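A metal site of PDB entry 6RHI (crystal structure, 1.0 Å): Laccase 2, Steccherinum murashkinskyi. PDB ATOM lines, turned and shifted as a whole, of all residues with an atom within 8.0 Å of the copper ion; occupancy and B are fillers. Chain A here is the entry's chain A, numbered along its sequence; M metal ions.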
ATOM      1  N   CYS A 208     -16.798  27.443  -2.789  1.00  0.00           N
ATOM      2  CA  CYS A 208     -18.092  27.024  -2.234  1.00  0.00           C
ATOM      3  C   CYS A 208     -19.207  27.076  -3.296  1.00  0.00           C
ATOM      4  O   CYS A 208     -20.300  26.552  -3.005  1.00  0.00           O
ATOM      5  CB  CYS A 208     -18.549  27.914  -1.077  1.00  0.00           C
ATOM      6  SG  CYS A 208     -18.013  27.116   0.513  1.00  0.00           S
ATOM      7  N   ASP A 209     -18.995  27.706  -4.445  1.00  0.00           N
ATOM      8  CA  ASP A 209     -20.099  27.863  -5.392  1.00  0.00           C
ATOM      9  C   ASP A 209     -19.630  28.144  -6.797  1.00  0.00           C
ATOM     10  O   ASP A 209     -19.774  27.274  -7.645  1.00  0.00           O
ATOM     11  CB  ASP A 209     -21.108  28.910  -4.860  1.00  0.00           C
ATOM     12  CG  ASP A 209     -22.221  29.248  -5.791  1.00  0.00           C
ATOM     13  OD1 ASP A 209     -22.238  28.903  -6.935  1.00  0.00           O
ATOM     14  OD2 ASP A 209     -23.067  30.093  -5.339  1.00  0.00           O
ATOM     15  N   PHE A 341     -33.336  21.065  -2.511  1.00  0.00           N
ATOM     16  CA  PHE A 341     -32.980  20.110  -3.532  1.00  0.00           C
ATOM     17  C   PHE A 341     -33.432  18.712  -3.100  1.00  0.00           C
ATOM     18  O   PHE A 341     -33.536  18.410  -1.909  1.00  0.00           O
ATOM     19  CB  PHE A 341     -31.473  20.106  -3.742  1.00  0.00           C
ATOM     20  CG  PHE A 341     -30.970  21.314  -4.455  1.00  0.00           C
ATOM     21  CD1 PHE A 341     -30.514  22.425  -3.767  1.00  0.00           C
ATOM     22  CD2 PHE A 341     -30.956  21.364  -5.827  1.00  0.00           C
ATOM     23  CE1 PHE A 341     -30.063  23.544  -4.419  1.00  0.00           C
ATOM     24  CE2 PHE A 341     -30.497  22.484  -6.508  1.00  0.00           C
ATOM     25  CZ  PHE A 341     -30.052  23.588  -5.824  1.00  0.00           C
ATOM     26  N   ALA A 392     -32.209  20.972 -12.833  1.00  0.00           N
ATOM     27  CA  ALA A 392     -32.506  21.610 -11.527  1.00  0.00           C
ATOM     28  C   ALA A 392     -31.902  22.995 -11.465  1.00  0.00           C
ATOM     29  O   ALA A 392     -30.758  23.212 -11.904  1.00  0.00           O
ATOM     30  CB  ALA A 392     -31.944  20.766 -10.371  1.00  0.00           C
ATOM     31  N   ALA A 393     -32.653  23.940 -10.912  1.00  0.00           N
ATOM     32  CA  ALA A 393     -32.184  25.336 -10.773  1.00  0.00           C
ATOM     33  C   ALA A 393     -30.838  25.398 -10.071  1.00  0.00           C
ATOM     34  O   ALA A 393     -30.447  24.538  -9.274  1.00  0.00           O
ATOM     35  CB  ALA A 393     -33.235  26.119  -9.977  1.00  0.00           C
ATOM     36  N   GLY A 394     -30.142  26.519 -10.332  1.00  0.00           N
ATOM     37  CA  GLY A 394     -28.888  26.791  -9.703  1.00  0.00           C
ATOM     38  C   GLY A 394     -27.709  26.157 -10.378  1.00  0.00           C
ATOM     39  O   GLY A 394     -26.616  26.200  -9.809  1.00  0.00           O
ATOM     40  N   GLY A 395     -27.889  25.637 -11.564  1.00  0.00           N
ATOM     41  CA  GLY A 395     -26.791  24.941 -12.294  1.00  0.00           C
ATOM     42  C   GLY A 395     -25.777  25.941 -12.863  1.00  0.00           C
ATOM     43  O   GLY A 395     -25.998  27.156 -12.847  1.00  0.00           O
ATOM     44  N   PRO A 396     -24.684  25.410 -13.436  1.00  0.00           N
ATOM     45  CA  PRO A 396     -24.385  24.004 -13.607  1.00  0.00           C
ATOM     46  C   PRO A 396     -23.819  23.405 -12.310  1.00  0.00           C
ATOM     47  O   PRO A 396     -22.942  23.978 -11.647  1.00  0.00           O
ATOM     48  CB  PRO A 396     -23.332  23.995 -14.708  1.00  0.00           C
ATOM     49  CG  PRO A 396     -22.691  25.341 -14.586  1.00  0.00           C
ATOM     50  CD  PRO A 396     -23.740  26.285 -14.136  1.00  0.00           C
ATOM     51  N   HIS A 397     -24.348  22.230 -11.939  1.00  0.00           N
ATOM     52  CA  HIS A 397     -24.031  21.597 -10.655  1.00  0.00           C
ATOM     53  C   HIS A 397     -22.828  20.684 -10.799  1.00  0.00           C
ATOM     54  O   HIS A 397     -22.865  19.726 -11.581  1.00  0.00           O
ATOM     55  CB  HIS A 397     -25.208  20.792 -10.149  1.00  0.00           C
ATOM     56  CG  HIS A 397     -26.448  21.601  -9.990  1.00  0.00           C
ATOM     57  ND1 HIS A 397     -26.633  22.435  -8.881  1.00  0.00           N
ATOM     58  CD2 HIS A 397     -27.580  21.649 -10.761  1.00  0.00           C
ATOM     59  CE1 HIS A 397     -27.830  22.980  -9.052  1.00  0.00           C
ATOM     60  NE2 HIS A 397     -28.405  22.555 -10.145  1.00  0.00           N
ATOM     61  N   PRO A 398     -21.756  20.902  -9.986  1.00  0.00           N
ATOM     62  CA  PRO A 398     -20.608  19.998 -10.005  1.00  0.00           C
ATOM     63  C   PRO A 398     -20.788  18.856  -8.993  1.00  0.00           C
ATOM     64  O   PRO A 398     -20.589  19.028  -7.783  1.00  0.00           O
ATOM     65  CB  PRO A 398     -19.460  20.923  -9.607  1.00  0.00           C
ATOM     66  CG  PRO A 398     -20.089  21.956  -8.697  1.00  0.00           C
ATOM     67  CD  PRO A 398     -21.503  22.119  -9.182  1.00  0.00           C
ATOM     68  N   PHE A 399     -21.155  17.693  -9.496  1.00  0.00           N
ATOM     69  CA  PHE A 399     -21.384  16.543  -8.634  1.00  0.00           C
ATOM     70  C   PHE A 399     -20.081  15.839  -8.316  1.00  0.00           C
ATOM     71  O   PHE A 399     -19.223  15.639  -9.157  1.00  0.00           O
ATOM     72  CB  PHE A 399     -22.412  15.555  -9.257  1.00  0.00           C
ATOM     73  CG  PHE A 399     -23.807  15.833  -8.765  1.00  0.00           C
ATOM     74  CD1 PHE A 399     -24.496  16.953  -9.151  1.00  0.00           C
ATOM     75  CD2 PHE A 399     -24.401  15.004  -7.812  1.00  0.00           C
ATOM     76  CE1 PHE A 399     -25.745  17.279  -8.617  1.00  0.00           C
ATOM     77  CE2 PHE A 399     -25.654  15.293  -7.303  1.00  0.00           C
ATOM     78  CZ  PHE A 399     -26.316  16.419  -7.702  1.00  0.00           C
ATOM     79  N   ILE A 430     -22.603  18.648 -14.296  1.00  0.00           N
ATOM     80  CA  ILE A 430     -23.666  17.919 -14.992  1.00  0.00           C
ATOM     81  C   ILE A 430     -24.331  18.745 -16.064  1.00  0.00           C
ATOM     82  O   ILE A 430     -25.226  18.280 -16.786  1.00  0.00           O
ATOM     83  CB  ILE A 430     -24.682  17.304 -14.022  1.00  0.00           C
ATOM     84  CG1 ILE A 430     -25.522  18.360 -13.323  1.00  0.00           C
ATOM     85  CG2 ILE A 430     -23.975  16.396 -13.014  1.00  0.00           C
ATOM     86  CD1 ILE A 430     -26.690  17.753 -12.525  1.00  0.00           C
ATOM     87  N   HIS A 452     -22.840  14.183  -3.932  1.00  0.00           N
ATOM     88  CA  HIS A 452     -23.560  15.425  -3.769  1.00  0.00           C
ATOM     89  C   HIS A 452     -23.055  16.482  -4.708  1.00  0.00           C
ATOM     90  O   HIS A 452     -21.935  16.425  -5.203  1.00  0.00           O
ATOM     91  CB  HIS A 452     -23.462  15.922  -2.295  1.00  0.00           C
ATOM     92  CG  HIS A 452     -22.066  16.218  -1.853  1.00  0.00           C
ATOM     93  ND1 HIS A 452     -21.453  17.435  -2.009  1.00  0.00           N
ATOM     94  CD2 HIS A 452     -21.182  15.453  -1.166  1.00  0.00           C
ATOM     95  CE1 HIS A 452     -20.248  17.387  -1.461  1.00  0.00           C
ATOM     96  NE2 HIS A 452     -20.024  16.178  -0.954  1.00  0.00           N
ATOM     97  N   CYS A 453     -23.890  17.509  -4.900  1.00  0.00           N
ATOM     98  CA  CYS A 453     -23.415  18.719  -5.530  1.00  0.00           C
ATOM     99  C   CYS A 453     -22.409  19.400  -4.625  1.00  0.00           C
ATOM    100  O   CYS A 453     -22.655  19.530  -3.416  1.00  0.00           O
ATOM    101  CB  CYS A 453     -24.588  19.668  -5.800  1.00  0.00           C
ATOM    102  SG  CYS A 453     -23.970  21.167  -6.660  1.00  0.00           S
ATOM    103  N   HIS A 454     -21.280  19.840  -5.183  1.00  0.00           N
ATOM    104  CA  HIS A 454     -20.227  20.484  -4.406  1.00  0.00           C
ATOM    105  C   HIS A 454     -20.381  22.003  -4.282  1.00  0.00           C
ATOM    106  O   HIS A 454     -19.530  22.635  -3.671  1.00  0.00           O
ATOM    107  CB  HIS A 454     -18.833  20.096  -4.903  1.00  0.00           C
ATOM    108  CG  HIS A 454     -17.817  19.945  -3.807  1.00  0.00           C
ATOM    109  ND1 HIS A 454     -17.430  20.975  -2.996  1.00  0.00           N
ATOM    110  CD2 HIS A 454     -17.092  18.891  -3.389  1.00  0.00           C
ATOM    111  CE1 HIS A 454     -16.521  20.523  -2.118  1.00  0.00           C
ATOM    112  NE2 HIS A 454     -16.293  19.245  -2.331  1.00  0.00           N
ATOM    113  N   ILE A 455     -21.487  22.559  -4.774  1.00  0.00           N
ATOM    114  CA  ILE A 455     -21.876  23.914  -4.368  1.00  0.00           C
ATOM    115  C   ILE A 455     -22.376  23.773  -2.940  1.00  0.00           C
ATOM    116  O   ILE A 455     -23.413  23.115  -2.710  1.00  0.00           O
ATOM    117  CB  ILE A 455     -22.879  24.514  -5.353  1.00  0.00           C
ATOM    118  CG1 ILE A 455     -22.261  24.711  -6.722  1.00  0.00           C
ATOM    119  CG2 ILE A 455     -23.425  25.834  -4.772  1.00  0.00           C
ATOM    120  CD1 ILE A 455     -23.213  25.035  -7.862  1.00  0.00           C
ATOM    121  N   ASP A 456     -21.629  24.323  -1.997  1.00  0.00           N
ATOM    122  CA  ASP A 456     -21.910  23.989  -0.601  1.00  0.00           C
ATOM    123  C   ASP A 456     -23.278  24.429  -0.145  1.00  0.00           C
ATOM    124  O   ASP A 456     -23.899  23.783   0.692  1.00  0.00           O
ATOM    125  CB  ASP A 456     -20.772  24.543   0.287  1.00  0.00           C
ATOM    126  CG  ASP A 456     -20.436  23.660   1.498  1.00  0.00           C
ATOM    127  OD1 ASP A 456     -20.541  22.426   1.363  1.00  0.00           O
ATOM    128  OD2 ASP A 456     -20.026  24.249   2.511  1.00  0.00           O
ATOM    129  N   TRP A 457     -23.762  25.540  -0.720  1.00  0.00           N
ATOM    130  CA  TRP A 457     -25.091  26.017  -0.399  1.00  0.00           C
ATOM    131  C   TRP A 457     -26.172  25.011  -0.857  1.00  0.00           C
ATOM    132  O   TRP A 457     -27.249  24.928  -0.267  1.00  0.00           O
ATOM    133  CB  TRP A 457     -25.334  27.412  -1.074  1.00  0.00           C
ATOM    134  CG  TRP A 457     -24.187  28.377  -0.847  1.00  0.00           C
ATOM    135  CD1 TRP A 457     -23.353  28.827  -1.823  1.00  0.00           C
ATOM    136  CD2 TRP A 457     -23.732  28.917   0.377  1.00  0.00           C
ATOM    137  NE1 TRP A 457     -22.406  29.663  -1.273  1.00  0.00           N
ATOM    138  CE2 TRP A 457     -22.602  29.740   0.085  1.00  0.00           C
ATOM    139  CE3 TRP A 457     -24.167  28.859   1.694  1.00  0.00           C
ATOM    140  CZ2 TRP A 457     -21.915  30.419   1.055  1.00  0.00           C
ATOM    141  CZ3 TRP A 457     -23.495  29.526   2.629  1.00  0.00           C
ATOM    142  CH2 TRP A 457     -22.372  30.307   2.328  1.00  0.00           C
ATOM    143  N   HIS A 458     -25.891  24.283  -1.931  1.00  0.00           N
ATOM    144  CA  HIS A 458     -26.837  23.278  -2.437  1.00  0.00           C
ATOM    145  C   HIS A 458     -26.794  21.994  -1.612  1.00  0.00           C
ATOM    146  O   HIS A 458     -27.834  21.391  -1.364  1.00  0.00           O
ATOM    147  CB  HIS A 458     -26.539  22.991  -3.935  1.00  0.00           C
ATOM    148  CG  HIS A 458     -26.703  24.169  -4.823  1.00  0.00           C
ATOM    149  ND1 HIS A 458     -26.394  24.078  -6.164  1.00  0.00           N
ATOM    150  CD2 HIS A 458     -27.131  25.427  -4.540  1.00  0.00           C
ATOM    151  CE1 HIS A 458     -26.659  25.269  -6.670  1.00  0.00           C
ATOM    152  NE2 HIS A 458     -27.093  26.109  -5.746  1.00  0.00           N
ATOM    153  N   LEU A 459     -25.585  21.580  -1.219  1.00  0.00           N
ATOM    154  CA  LEU A 459     -25.476  20.463  -0.275  1.00  0.00           C
ATOM    155  C   LEU A 459     -26.274  20.770   0.970  1.00  0.00           C
ATOM    156  O   LEU A 459     -27.042  19.908   1.477  1.00  0.00           O
ATOM    157  CB  LEU A 459     -24.021  20.220   0.049  1.00  0.00           C
ATOM    158  CG  LEU A 459     -23.722  19.239   1.185  1.00  0.00           C
ATOM    159  CD1 LEU A 459     -24.326  17.867   0.919  1.00  0.00           C
ATOM    160  CD2 LEU A 459     -22.229  19.106   1.428  1.00  0.00           C
ATOM    161  N   PHE A 463     -28.953  18.562  -1.521  1.00  0.00           N
ATOM    162  CA  PHE A 463     -28.645  17.964  -2.855  1.00  0.00           C
ATOM    163  C   PHE A 463     -27.594  16.850  -2.723  1.00  0.00           C
ATOM    164  O   PHE A 463     -26.447  16.994  -3.142  1.00  0.00           O
ATOM    165  CB  PHE A 463     -28.251  19.040  -3.828  1.00  0.00           C
ATOM    166  CG  PHE A 463     -28.597  18.801  -5.300  1.00  0.00           C
ATOM    167  CD1 PHE A 463     -29.502  17.840  -5.726  1.00  0.00           C
ATOM    168  CD2 PHE A 463     -28.084  19.659  -6.243  1.00  0.00           C
ATOM    169  CE1 PHE A 463     -29.900  17.753  -7.052  1.00  0.00           C
ATOM    170  CE2 PHE A 463     -28.460  19.586  -7.586  1.00  0.00           C
ATOM    171  CZ  PHE A 463     -29.387  18.656  -7.974  1.00  0.00           C
HETATM  172 CU    CU M   1     -25.619  22.501  -7.133  1.00  0.00          CU
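SG of Cys 453 sits close to N of Ile 455 (3.4 Å). The backbone carbonyl oxygen (O) of Phe 463 is in hydrogen-bond range of the backbone NH (N) of Cys 453 (3.1 Å). The backbone carbonyl oxygen of His 458 lies within hydrogen-bond range of the backbone NH of Phe 463 (3.0 Å). The backbone carbonyl oxygen (O) of His 397 lies within hydrogen-bond range of the backbone NH (N) of Ile 430 (2.9 Å). The backbone carbonyl oxygen of Ala 392 is in hydrogen-bond range of a ring nitrogen (NE2) of His 397, at 3.0 Å. NE2 of His 397 sits at hydrogen-bond distance from N of Gly 395 (3.4 Å). NE2 of His 397 is in hydrogen-bond range of O of Ala 393 (3.0 Å).
Residues that only touch the copper ion: Ile 455 (3.6 Å) and Phe 463 (3.9 Å). Of the 21 residues printed, 5 come within 4 Å of the copper ion.
The copper ion is bound by a ring nitrogen (ND1) of His 458 (2.0 Å), a ring nitrogen (ND1) of His 397 (2.0 Å) and the side-chain sulfur of Cys 453 (2.2 Å).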
